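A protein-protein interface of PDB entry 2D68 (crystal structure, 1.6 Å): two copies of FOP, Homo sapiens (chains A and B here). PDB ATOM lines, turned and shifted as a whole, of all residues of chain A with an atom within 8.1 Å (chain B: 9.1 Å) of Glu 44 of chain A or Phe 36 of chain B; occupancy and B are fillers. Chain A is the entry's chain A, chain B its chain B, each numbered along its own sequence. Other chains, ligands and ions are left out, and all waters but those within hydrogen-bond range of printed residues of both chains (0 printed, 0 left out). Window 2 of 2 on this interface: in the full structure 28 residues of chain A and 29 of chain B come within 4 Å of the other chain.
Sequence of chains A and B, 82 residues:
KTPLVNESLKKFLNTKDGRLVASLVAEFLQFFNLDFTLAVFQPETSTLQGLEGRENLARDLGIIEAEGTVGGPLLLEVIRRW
The backbone carbonyl oxygen (O) of Phe 32 of chain B is in hydrogen-bond range of the side-chain amide nitrogen (ND2) of Asn 6 of chain A (2.8 Å). The side-chain carboxylate (OE2) of Glu 44 of chain A sits at hydrogen-bond distance from the backbone NH (N) of Phe 36 of chain B (3.1 Å). The backbone NH (N) of Asp 35 of chain B lies within hydrogen-bond range of the side-chain carboxylate (OE2) of Glu 44 of chain A (3.2 Å). The side-chain carboxylate (OE1) of Glu 44 of chain A sits at hydrogen-bond distance from the side-chain hydroxyl (OG1) of Thr 37 of chain B (2.5 Å). The backbone carbonyl oxygen of Leu 34 of chain B sits close to the side-chain carboxylate of Glu 44 of chain A (3.4 Å). OG1 of Thr 37 of chain A lies close to N of Phe 41 of chain B, at 3.4 Å.
N of Leu 34 of chain B sits at hydrogen-bond distance from O of Leu 29 of chain B (2.9 Å). The side-chain amide oxygen of Asn 6 of chain A sits at hydrogen-bond distance from the backbone NH of Leu 9 of chain A. The side-chain hydroxyl of Thr 45 of chain A is in hydrogen-bond range of the backbone carbonyl oxygen of Phe 41 of chain A (2.7 Å). OG1 of Thr 45 of chain A is in hydrogen-bond range of OG1 of Thr 47 of chain A (2.7 Å). O of Gln 42 of chain A lies within hydrogen-bond range of OG1 of Thr 45 of chain A.
Among the printed residues, merely in contact across the chains: Leu 9 of chain A with Phe 32 of chain B (3.8 Å), Phe 36 of chain A with Val 40 of chain B (3.5 Å), Thr 37 of chain A with Thr 37 of chain B (3.6 Å), Thr 37 of chain A with Val 40 of chain B (3.5 Å), Val 40 of chain A with Phe 36 of chain B (3.6 Å), Val 40 of chain A with Thr 37 of chain B (3.4 Å), Phe 41 of chain A with Thr 37 of chain B (3.4 Å) and Thr 45 of chain A with Leu 34 of chain B (3.7 Å).
Val 5 of chain A touches none of the printed residues of chain B. Of the printed residues of chain B, Val 40 of chain A touches Phe 36 and Thr 37. No residue of chain B comes within 4 Å of Pro 43 of chain A. Glu 44 of chain A touches just these residues of chain B: Leu 34 (3.2 Å), Asp 35 (3.2 Å), Phe 36 (3.1 Å) and Thr 37 (2.5 Å). Phe 28 of chain B touches none of the printed residues of chain A. Printed residues of chain A within 4 Å of Leu 34 of chain B: Glu 44 and Thr 45. Of the printed residues of chain A, Asp 35 of chain B touches Glu 44 (3.2 Å). Of the printed residues of chain A, Phe 41 of chain B touches Thr 37 (3.3 Å). The nearest residue of chain B that does not touch Glu 44 of chain A is Asn 33 of chain B (4.1 Å). The nearest printed residue of chain B that does not touch Phe 36 of chain A is Phe 41 of chain B (6.3 Å).
Of the 15 printed residues of chain B, 7 touch a printed residue of chain A. Hydrophobic or aromatic side chains of chain B that line the printed part of chain A: Phe 32, Leu 34, Phe 36, Val 40 and Phe 41. Hydrophobic or aromatic side chains of chain A that line the printed part of chain B: Leu 9, Phe 36, Val 40 and Phe 41. Along chain A the printed residues that touch a printed residue of chain B span positions 6 to 45. Among the printed residues, no Asp or Glu carboxylate lies within 4 Å of a Lys or Arg side-chain nitrogen of the other chain.
Phe 36 of chain A touches Val 40 of chain B, and with the chains exchanged Val 40 of chain A touches Phe 36 of chain B. Thr 37 of chain B touches its own counterpart, Thr 37 of chain A. Thr 37 of chain A touches Val 40 of chain B, and with the chains exchanged Val 40 of chain A touches Thr 37 of chain B. Thr 37 of chain A touches Phe 41 of chain B, and with the chains exchanged Phe 41 of chain A touches Thr 37 of chain B.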
ATOM      1  N   VAL A   5       6.753 -38.468 -13.308  1.00  0.00           N
ATOM      2  CA  VAL A   5       6.406 -37.915 -11.965  1.00  0.00           C
ATOM      3  C   VAL A   5       7.568 -37.986 -10.961  1.00  0.00           C
ATOM      4  O   VAL A   5       8.293 -38.991 -10.873  1.00  0.00           O
ATOM      5  CB  VAL A   5       5.128 -38.573 -11.366  1.00  0.00           C
ATOM      6  CG1 VAL A   5       3.879 -38.180 -12.171  1.00  0.00           C
ATOM      7  CG2 VAL A   5       5.272 -40.100 -11.276  1.00  0.00           C
ATOM      8  N   ASN A   6       7.719 -36.899 -10.207  1.00  0.00           N
ATOM      9  CA  ASN A   6       8.766 -36.740  -9.202  1.00  0.00           C
ATOM     10  C   ASN A   6       8.299 -37.230  -7.816  1.00  0.00           C
ATOM     11  O   ASN A   6       7.456 -36.595  -7.191  1.00  0.00           O
ATOM     12  CB  ASN A   6       9.135 -35.254  -9.149  1.00  0.00           C
ATOM     13  CG  ASN A   6      10.405 -34.976  -8.369  1.00  0.00           C
ATOM     14  OD1 ASN A   6      10.692 -35.603  -7.335  1.00  0.00           O
ATOM     15  ND2 ASN A   6      11.167 -34.002  -8.854  1.00  0.00           N
ATOM     16  N   LEU A   9       9.029 -34.994  -4.760  1.00  0.00           N
ATOM     17  CA  LEU A   9       8.075 -33.883  -4.878  1.00  0.00           C
ATOM     18  C   LEU A   9       6.616 -34.282  -4.621  1.00  0.00           C
ATOM     19  O   LEU A   9       5.854 -33.528  -3.991  1.00  0.00           O
ATOM     20  CB  LEU A   9       8.207 -33.207  -6.247  1.00  0.00           C
ATOM     21  CG  LEU A   9       7.333 -31.979  -6.474  1.00  0.00           C
ATOM     22  CD1 LEU A   9       7.671 -30.830  -5.528  1.00  0.00           C
ATOM     23  CD2 LEU A   9       7.498 -31.548  -7.909  1.00  0.00           C
ATOM     24  N   LEU A  13       4.327 -32.556  -1.863  1.00  0.00           N
ATOM     25  CA  LEU A  13       3.057 -31.927  -2.196  1.00  0.00           C
ATOM     26  C   LEU A  13       1.881 -32.496  -1.410  1.00  0.00           C
ATOM     27  O   LEU A  13       0.838 -31.838  -1.308  1.00  0.00           O
ATOM     28  CB  LEU A  13       2.785 -32.066  -3.696  1.00  0.00           C
ATOM     29  CG  LEU A  13       3.698 -31.217  -4.580  1.00  0.00           C
ATOM     30  CD1 LEU A  13       3.467 -31.587  -6.033  1.00  0.00           C
ATOM     31  CD2 LEU A  13       3.485 -29.725  -4.348  1.00  0.00           C
ATOM     32  N   PHE A  36       6.312 -18.177 -19.198  1.00  0.00           N
ATOM     33  CA  PHE A  36       7.038 -19.299 -19.796  1.00  0.00           C
ATOM     34  C   PHE A  36       7.511 -20.260 -18.713  1.00  0.00           C
ATOM     35  O   PHE A  36       7.449 -21.482 -18.886  1.00  0.00           O
ATOM     36  CB  PHE A  36       8.181 -18.807 -20.689  1.00  0.00           C
ATOM     37  CG  PHE A  36       7.697 -18.132 -21.941  1.00  0.00           C
ATOM     38  CD1 PHE A  36       7.006 -18.861 -22.917  1.00  0.00           C
ATOM     39  CD2 PHE A  36       7.896 -16.779 -22.135  1.00  0.00           C
ATOM     40  CE1 PHE A  36       6.529 -18.232 -24.070  1.00  0.00           C
ATOM     41  CE2 PHE A  36       7.435 -16.140 -23.295  1.00  0.00           C
ATOM     42  CZ  PHE A  36       6.743 -16.863 -24.258  1.00  0.00           C
ATOM     43  N   THR A  37       7.944 -19.706 -17.576  1.00  0.00           N
ATOM     44  CA  THR A  37       8.333 -20.538 -16.444  1.00  0.00           C
ATOM     45  C   THR A  37       7.150 -21.360 -15.955  1.00  0.00           C
ATOM     46  O   THR A  37       7.297 -22.565 -15.697  1.00  0.00           O
ATOM     47  CB  THR A  37       8.931 -19.687 -15.302  1.00  0.00           C
ATOM     48  OG1 THR A  37      10.062 -18.985 -15.813  1.00  0.00           O
ATOM     49  CG2 THR A  37       9.376 -20.581 -14.143  1.00  0.00           C
ATOM     50  N   LEU A  38       5.981 -20.726 -15.857  1.00  0.00           N
ATOM     51  CA  LEU A  38       4.780 -21.441 -15.448  1.00  0.00           C
ATOM     52  C   LEU A  38       4.428 -22.568 -16.409  1.00  0.00           C
ATOM     53  O   LEU A  38       3.955 -23.623 -15.967  1.00  0.00           O
ATOM     54  CB  LEU A  38       3.606 -20.469 -15.284  1.00  0.00           C
ATOM     55  CG  LEU A  38       3.617 -19.677 -13.970  1.00  0.00           C
ATOM     56  CD1 LEU A  38       2.706 -18.469 -14.095  1.00  0.00           C
ATOM     57  CD2 LEU A  38       3.194 -20.549 -12.782  1.00  0.00           C
ATOM     58  N   ALA A  39       4.662 -22.349 -17.708  1.00  0.00           N
ATOM     59  CA  ALA A  39       4.330 -23.346 -18.730  1.00  0.00           C
ATOM     60  C   ALA A  39       5.109 -24.648 -18.552  1.00  0.00           C
ATOM     61  O   ALA A  39       4.625 -25.729 -18.918  1.00  0.00           O
ATOM     62  CB  ALA A  39       4.555 -22.769 -20.123  1.00  0.00           C
ATOM     63  N   VAL A  40       6.322 -24.537 -18.003  1.00  0.00           N
ATOM     64  CA  VAL A  40       7.143 -25.702 -17.690  1.00  0.00           C
ATOM     65  C   VAL A  40       6.926 -26.207 -16.255  1.00  0.00           C
ATOM     66  O   VAL A  40       6.925 -27.413 -16.013  1.00  0.00           O
ATOM     67  CB  VAL A  40       8.630 -25.423 -17.956  1.00  0.00           C
ATOM     68  CG1 VAL A  40       9.469 -26.618 -17.592  1.00  0.00           C
ATOM     69  CG2 VAL A  40       8.851 -25.069 -19.439  1.00  0.00           C
ATOM     70  N   PHE A  41       6.723 -25.278 -15.326  1.00  0.00           N
ATOM     71  CA  PHE A  41       6.502 -25.611 -13.919  1.00  0.00           C
ATOM     72  C   PHE A  41       5.314 -26.550 -13.738  1.00  0.00           C
ATOM     73  O   PHE A  41       5.414 -27.548 -13.026  1.00  0.00           O
ATOM     74  CB  PHE A  41       6.293 -24.316 -13.127  1.00  0.00           C
ATOM     75  CG  PHE A  41       6.016 -24.517 -11.661  1.00  0.00           C
ATOM     76  CD1 PHE A  41       7.055 -24.685 -10.750  1.00  0.00           C
ATOM     77  CD2 PHE A  41       4.702 -24.472 -11.192  1.00  0.00           C
ATOM     78  CE1 PHE A  41       6.777 -24.845  -9.371  1.00  0.00           C
ATOM     79  CE2 PHE A  41       4.420 -24.643  -9.836  1.00  0.00           C
ATOM     80  CZ  PHE A  41       5.456 -24.818  -8.932  1.00  0.00           C
ATOM     81  N   GLN A  42       4.203 -26.231 -14.401  1.00  0.00           N
ATOM     82  CA  GLN A  42       2.983 -27.006 -14.283  1.00  0.00           C
ATOM     83  C   GLN A  42       3.204 -28.504 -14.643  1.00  0.00           C
ATOM     84  O   GLN A  42       3.009 -29.380 -13.790  1.00  0.00           O
ATOM     85  CB  GLN A  42       1.831 -26.302 -15.026  1.00  0.00           C
ATOM     86  CG  GLN A  42       1.395 -25.014 -14.271  1.00  0.00           C
ATOM     87  CD  GLN A  42       0.745 -23.905 -15.113  1.00  0.00           C
ATOM     88  OE1 GLN A  42       0.424 -22.837 -14.577  1.00  0.00           O
ATOM     89  NE2 GLN A  42       0.575 -24.130 -16.409  1.00  0.00           N
ATOM     90  N   PRO A  43       3.670 -28.809 -15.867  1.00  0.00           N
ATOM     91  CA  PRO A  43       3.947 -30.227 -16.125  1.00  0.00           C
ATOM     92  C   PRO A  43       5.113 -30.850 -15.351  1.00  0.00           C
ATOM     93  O   PRO A  43       5.057 -32.048 -15.047  1.00  0.00           O
ATOM     94  CB  PRO A  43       4.216 -30.273 -17.637  1.00  0.00           C
ATOM     95  CG  PRO A  43       4.636 -28.877 -17.999  1.00  0.00           C
ATOM     96  CD  PRO A  43       3.900 -27.973 -17.058  1.00  0.00           C
ATOM     97  N   GLU A  44       6.155 -30.079 -15.029  1.00  0.00           N
ATOM     98  CA  GLU A  44       7.324 -30.683 -14.398  1.00  0.00           C
ATOM     99  C   GLU A  44       6.984 -31.085 -12.964  1.00  0.00           C
ATOM    100  O   GLU A  44       7.569 -32.041 -12.425  1.00  0.00           O
ATOM    101  CB  GLU A  44       8.566 -29.774 -14.461  1.00  0.00           C
ATOM    102  CG  GLU A  44       9.895 -30.536 -14.276  1.00  0.00           C
ATOM    103  CD  GLU A  44      11.128 -29.701 -14.534  1.00  0.00           C
ATOM    104  OE1 GLU A  44      11.101 -28.477 -14.279  1.00  0.00           O
ATOM    105  OE2 GLU A  44      12.144 -30.273 -14.984  1.00  0.00           O
ATOM    106  N   THR A  45       6.039 -30.366 -12.356  1.00  0.00           N
ATOM    107  CA  THR A  45       5.622 -30.645 -10.967  1.00  0.00           C
ATOM    108  C   THR A  45       4.346 -31.482 -10.843  1.00  0.00           C
ATOM    109  O   THR A  45       3.937 -31.846  -9.730  1.00  0.00           O
ATOM    110  CB  THR A  45       5.369 -29.344 -10.184  1.00  0.00           C
ATOM    111  OG1 THR A  45       4.287 -28.633 -10.804  1.00  0.00           O
ATOM    112  CG2 THR A  45       6.616 -28.455 -10.154  1.00  0.00           C
ATOM    113  N   SER A  46       3.713 -31.770 -11.981  1.00  0.00           N
ATOM    114  CA  SER A  46       2.414 -32.451 -12.012  1.00  0.00           C
ATOM    115  C   SER A  46       1.335 -31.702 -11.215  1.00  0.00           C
ATOM    116  O   SER A  46       0.441 -32.324 -10.632  1.00  0.00           O
ATOM    117  CB  SER A  46       2.554 -33.909 -11.534  1.00  0.00           C
ATOM    118  OG  SER A  46       3.625 -34.549 -12.208  1.00  0.00           O
ATOM    119  N   THR A  47       1.422 -30.371 -11.189  1.00  0.00           N
ATOM    120  CA  THR A  47       0.425 -29.540 -10.500  1.00  0.00           C
ATOM    121  C   THR A  47      -0.524 -28.865 -11.498  1.00  0.00           C
ATOM    122  O   THR A  47      -0.151 -27.909 -12.200  1.00  0.00           O
ATOM    123  CB  THR A  47       1.072 -28.487  -9.549  1.00  0.00           C
ATOM    124  OG1 THR A  47       1.883 -27.568 -10.299  1.00  0.00           O
ATOM    125  CG2 THR A  47       1.924 -29.160  -8.466  1.00  0.00           C
ATOM    126  N   PHE B  28      14.137 -23.787  -4.274  1.00  0.00           N
ATOM    127  CA  PHE B  28      13.081 -24.777  -4.322  1.00  0.00           C
ATOM    128  C   PHE B  28      13.143 -25.568  -5.643  1.00  0.00           C
ATOM    129  O   PHE B  28      13.067 -26.797  -5.642  1.00  0.00           O
ATOM    130  CB  PHE B  28      11.714 -24.095  -4.145  1.00  0.00           C
ATOM    131  CG  PHE B  28      10.561 -25.004  -4.424  1.00  0.00           C
ATOM    132  CD1 PHE B  28       9.969 -25.739  -3.410  1.00  0.00           C
ATOM    133  CD2 PHE B  28      10.042 -25.125  -5.717  1.00  0.00           C
ATOM    134  CE1 PHE B  28       8.909 -26.603  -3.692  1.00  0.00           C
ATOM    135  CE2 PHE B  28       8.982 -25.979  -5.989  1.00  0.00           C
ATOM    136  CZ  PHE B  28       8.419 -26.716  -4.972  1.00  0.00           C
ATOM    137  N   LEU B  29      13.302 -24.859  -6.759  1.00  0.00           N
ATOM    138  CA  LEU B  29      13.386 -25.524  -8.065  1.00  0.00           C
ATOM    139  C   LEU B  29      14.585 -26.455  -8.112  1.00  0.00           C
ATOM    140  O   LEU B  29      14.489 -27.602  -8.587  1.00  0.00           O
ATOM    141  CB  LEU B  29      13.444 -24.489  -9.203  1.00  0.00           C
ATOM    142  CG  LEU B  29      12.260 -23.531  -9.304  1.00  0.00           C
ATOM    143  CD1 LEU B  29      12.573 -22.480 -10.406  1.00  0.00           C
ATOM    144  CD2 LEU B  29      10.966 -24.265  -9.629  1.00  0.00           C
ATOM    145  N   GLN B  30      15.721 -25.993  -7.601  1.00  0.00           N
ATOM    146  CA  GLN B  30      16.936 -26.829  -7.591  1.00  0.00           C
ATOM    147  C   GLN B  30      16.789 -28.038  -6.675  1.00  0.00           C
ATOM    148  O   GLN B  30      17.165 -29.174  -7.042  1.00  0.00           O
ATOM    149  CB  GLN B  30      18.162 -25.982  -7.253  1.00  0.00           C
ATOM    150  CG  GLN B  30      18.369 -24.899  -8.317  1.00  0.00           C
ATOM    151  CD  GLN B  30      19.763 -24.322  -8.373  1.00  0.00           C
ATOM    152  OE1 GLN B  30      19.966 -23.159  -8.036  1.00  0.00           O
ATOM    153  NE2 GLN B  30      20.720 -25.113  -8.845  1.00  0.00           N
ATOM    154  N   PHE B  32      14.226 -29.833  -5.933  1.00  0.00           N
ATOM    155  CA  PHE B  32      13.401 -30.890  -6.516  1.00  0.00           C
ATOM    156  C   PHE B  32      13.792 -31.237  -7.951  1.00  0.00           C
ATOM    157  O   PHE B  32      13.034 -31.898  -8.670  1.00  0.00           O
ATOM    158  CB  PHE B  32      11.919 -30.555  -6.386  1.00  0.00           C
ATOM    159  CG  PHE B  32      11.412 -30.699  -4.989  1.00  0.00           C
ATOM    160  CD1 PHE B  32      11.356 -31.960  -4.394  1.00  0.00           C
ATOM    161  CD2 PHE B  32      11.028 -29.579  -4.247  1.00  0.00           C
ATOM    162  CE1 PHE B  32      10.925 -32.116  -3.086  1.00  0.00           C
ATOM    163  CE2 PHE B  32      10.575 -29.728  -2.928  1.00  0.00           C
ATOM    164  CZ  PHE B  32      10.507 -31.000  -2.360  1.00  0.00           C
ATOM    165  N   ASN B  33      14.993 -30.825  -8.345  1.00  0.00           N
ATOM    166  CA  ASN B  33      15.504 -31.122  -9.696  1.00  0.00           C
ATOM    167  C   ASN B  33      14.536 -30.717 -10.798  1.00  0.00           C
ATOM    168  O   ASN B  33      14.347 -31.448 -11.787  1.00  0.00           O
ATOM    169  CB  ASN B  33      15.864 -32.600  -9.807  1.00  0.00           C
ATOM    170  CG  ASN B  33      16.903 -33.010  -8.786  1.00  0.00           C
ATOM    171  OD1 ASN B  33      16.653 -33.881  -7.959  1.00  0.00           O
ATOM    172  ND2 ASN B  33      18.051 -32.371  -8.819  1.00  0.00           N
ATOM    173  N   LEU B  34      13.929 -29.538 -10.634  1.00  0.00           N
ATOM    174  CA  LEU B  34      13.002 -29.012 -11.635  1.00  0.00           C
ATOM    175  C   LEU B  34      13.848 -28.255 -12.662  1.00  0.00           C
ATOM    176  O   LEU B  34      13.810 -27.016 -12.768  1.00  0.00           O
ATOM    177  CB  LEU B  34      11.942 -28.144 -10.959  1.00  0.00           C
ATOM    178  CG  LEU B  34      11.106 -28.901  -9.916  1.00  0.00           C
ATOM    179  CD1 LEU B  34      10.168 -27.984  -9.171  1.00  0.00           C
ATOM    180  CD2 LEU B  34      10.308 -30.051 -10.526  1.00  0.00           C
ATOM    181  N   ASP B  35      14.638 -29.032 -13.400  1.00  0.00           N
ATOM    182  CA  ASP B  35      15.730 -28.497 -14.194  1.00  0.00           C
ATOM    183  C   ASP B  35      15.243 -27.748 -15.439  1.00  0.00           C
ATOM    184  O   ASP B  35      15.845 -26.747 -15.840  1.00  0.00           O
ATOM    185  CB  ASP B  35      16.738 -29.612 -14.520  1.00  0.00           C
ATOM    186  CG  ASP B  35      17.346 -30.223 -13.263  1.00  0.00           C
ATOM    187  OD1 ASP B  35      17.722 -29.463 -12.355  1.00  0.00           O
ATOM    188  OD2 ASP B  35      17.438 -31.461 -13.187  1.00  0.00           O
ATOM    189  N   PHE B  36      14.153 -28.221 -16.043  1.00  0.00           N
ATOM    190  CA  PHE B  36      13.606 -27.514 -17.194  1.00  0.00           C
ATOM    191  C   PHE B  36      12.935 -26.212 -16.760  1.00  0.00           C
ATOM    192  O   PHE B  36      13.068 -25.180 -17.428  1.00  0.00           O
ATOM    193  CB  PHE B  36      12.683 -28.420 -17.997  1.00  0.00           C
ATOM    194  CG  PHE B  36      13.393 -29.613 -18.589  1.00  0.00           C
ATOM    195  CD1 PHE B  36      14.346 -29.438 -19.588  1.00  0.00           C
ATOM    196  CD2 PHE B  36      13.116 -30.898 -18.142  1.00  0.00           C
ATOM    197  CE1 PHE B  36      15.019 -30.540 -20.136  1.00  0.00           C
ATOM    198  CE2 PHE B  36      13.781 -32.012 -18.689  1.00  0.00           C
ATOM    199  CZ  PHE B  36      14.730 -31.829 -19.676  1.00  0.00           C
ATOM    200  N   THR B  37      12.237 -26.253 -15.617  1.00  0.00           N
ATOM    201  CA  THR B  37      11.711 -25.015 -15.066  1.00  0.00           C
ATOM    202  C   THR B  37      12.822 -24.002 -14.797  1.00  0.00           C
ATOM    203  O   THR B  37      12.688 -22.835 -15.156  1.00  0.00           O
ATOM    204  CB  THR B  37      10.904 -25.265 -13.778  1.00  0.00           C
ATOM    205  OG1 THR B  37       9.889 -26.247 -14.036  1.00  0.00           O
ATOM    206  CG2 THR B  37      10.221 -24.003 -13.351  1.00  0.00           C
ATOM    207  N   LEU B  38      13.926 -24.435 -14.181  1.00  0.00           N
ATOM    208  CA  LEU B  38      15.051 -23.532 -13.943  1.00  0.00           C
ATOM    209  C   LEU B  38      15.623 -22.959 -15.246  1.00  0.00           C
ATOM    210  O   LEU B  38      15.973 -21.785 -15.305  1.00  0.00           O
ATOM    211  CB  LEU B  38      16.143 -24.240 -13.135  1.00  0.00           C
ATOM    212  CG  LEU B  38      17.263 -23.365 -12.595  1.00  0.00           C
ATOM    213  CD1 LEU B  38      16.688 -22.388 -11.560  1.00  0.00           C
ATOM    214  CD2 LEU B  38      18.303 -24.274 -11.965  1.00  0.00           C
ATOM    215  N   ALA B  39      15.680 -23.795 -16.278  1.00  0.00           N
ATOM    216  CA  ALA B  39      16.217 -23.410 -17.581  1.00  0.00           C
ATOM    217  C   ALA B  39      15.442 -22.250 -18.210  1.00  0.00           C
ATOM    218  O   ALA B  39      16.007 -21.482 -18.997  1.00  0.00           O
ATOM    219  CB  ALA B  39      16.219 -24.611 -18.504  1.00  0.00           C
ATOM    220  N   VAL B  40      14.149 -22.154 -17.890  1.00  0.00           N
ATOM    221  CA  VAL B  40      13.314 -21.033 -18.367  1.00  0.00           C
ATOM    222  C   VAL B  40      13.280 -19.888 -17.357  1.00  0.00           C
ATOM    223  O   VAL B  40      13.331 -18.707 -17.734  1.00  0.00           O
ATOM    224  CB  VAL B  40      11.887 -21.519 -18.706  1.00  0.00           C
ATOM    225  CG1 VAL B  40      10.980 -20.372 -19.156  1.00  0.00           C
ATOM    226  CG2 VAL B  40      11.954 -22.556 -19.791  1.00  0.00           C
ATOM    227  N   PHE B  41      13.209 -20.242 -16.077  1.00  0.00           N
ATOM    228  CA  PHE B  41      13.250 -19.247 -14.982  1.00  0.00           C
ATOM    229  C   PHE B  41      14.431 -18.282 -15.087  1.00  0.00           C
ATOM    230  O   PHE B  41      14.271 -17.067 -14.952  1.00  0.00           O
ATOM    231  CB  PHE B  41      13.295 -19.979 -13.642  1.00  0.00           C
ATOM    232  CG  PHE B  41      13.301 -19.077 -12.425  1.00  0.00           C
ATOM    233  CD1 PHE B  41      12.110 -18.632 -11.868  1.00  0.00           C
ATOM    234  CD2 PHE B  41      14.507 -18.713 -11.818  1.00  0.00           C
ATOM    235  CE1 PHE B  41      12.107 -17.824 -10.719  1.00  0.00           C
ATOM    236  CE2 PHE B  41      14.513 -17.900 -10.676  1.00  0.00           C
ATOM    237  CZ  PHE B  41      13.312 -17.456 -10.131  1.00  0.00           C
ATOM    238  N   GLN B  42      15.617 -18.825 -15.322  1.00  0.00           N
ATOM    239  CA  GLN B  42      16.810 -17.988 -15.362  1.00  0.00           C
ATOM    240  C   GLN B  42      16.786 -16.907 -16.466  1.00  0.00           C
ATOM    241  O   GLN B  42      16.963 -15.720 -16.162  1.00  0.00           O
ATOM    242  CB  GLN B  42      18.060 -18.849 -15.335  1.00  0.00           C
ATOM    243  CG  GLN B  42      18.154 -19.638 -14.014  1.00  0.00           C
ATOM    244  CD  GLN B  42      19.493 -20.292 -13.804  1.00  0.00           C
ATOM    245  OE1 GLN B  42      20.092 -20.841 -14.740  1.00  0.00           O
ATOM    246  NE2 GLN B  42      19.969 -20.267 -12.559  1.00  0.00           N
ATOM    247  N   PRO B  43      16.550 -17.288 -17.742  1.00  0.00           N
ATOM    248  CA  PRO B  43      16.444 -16.191 -18.715  1.00  0.00           C
ATOM    249  C   PRO B  43      15.215 -15.297 -18.491  1.00  0.00           C
ATOM    250  O   PRO B  43      15.291 -14.087 -18.728  1.00  0.00           O
ATOM    251  CB  PRO B  43      16.340 -16.910 -20.080  1.00  0.00           C
ATOM    252  CG  PRO B  43      15.921 -18.289 -19.768  1.00  0.00           C
ATOM    253  CD  PRO B  43      16.422 -18.609 -18.380  1.00  0.00           C
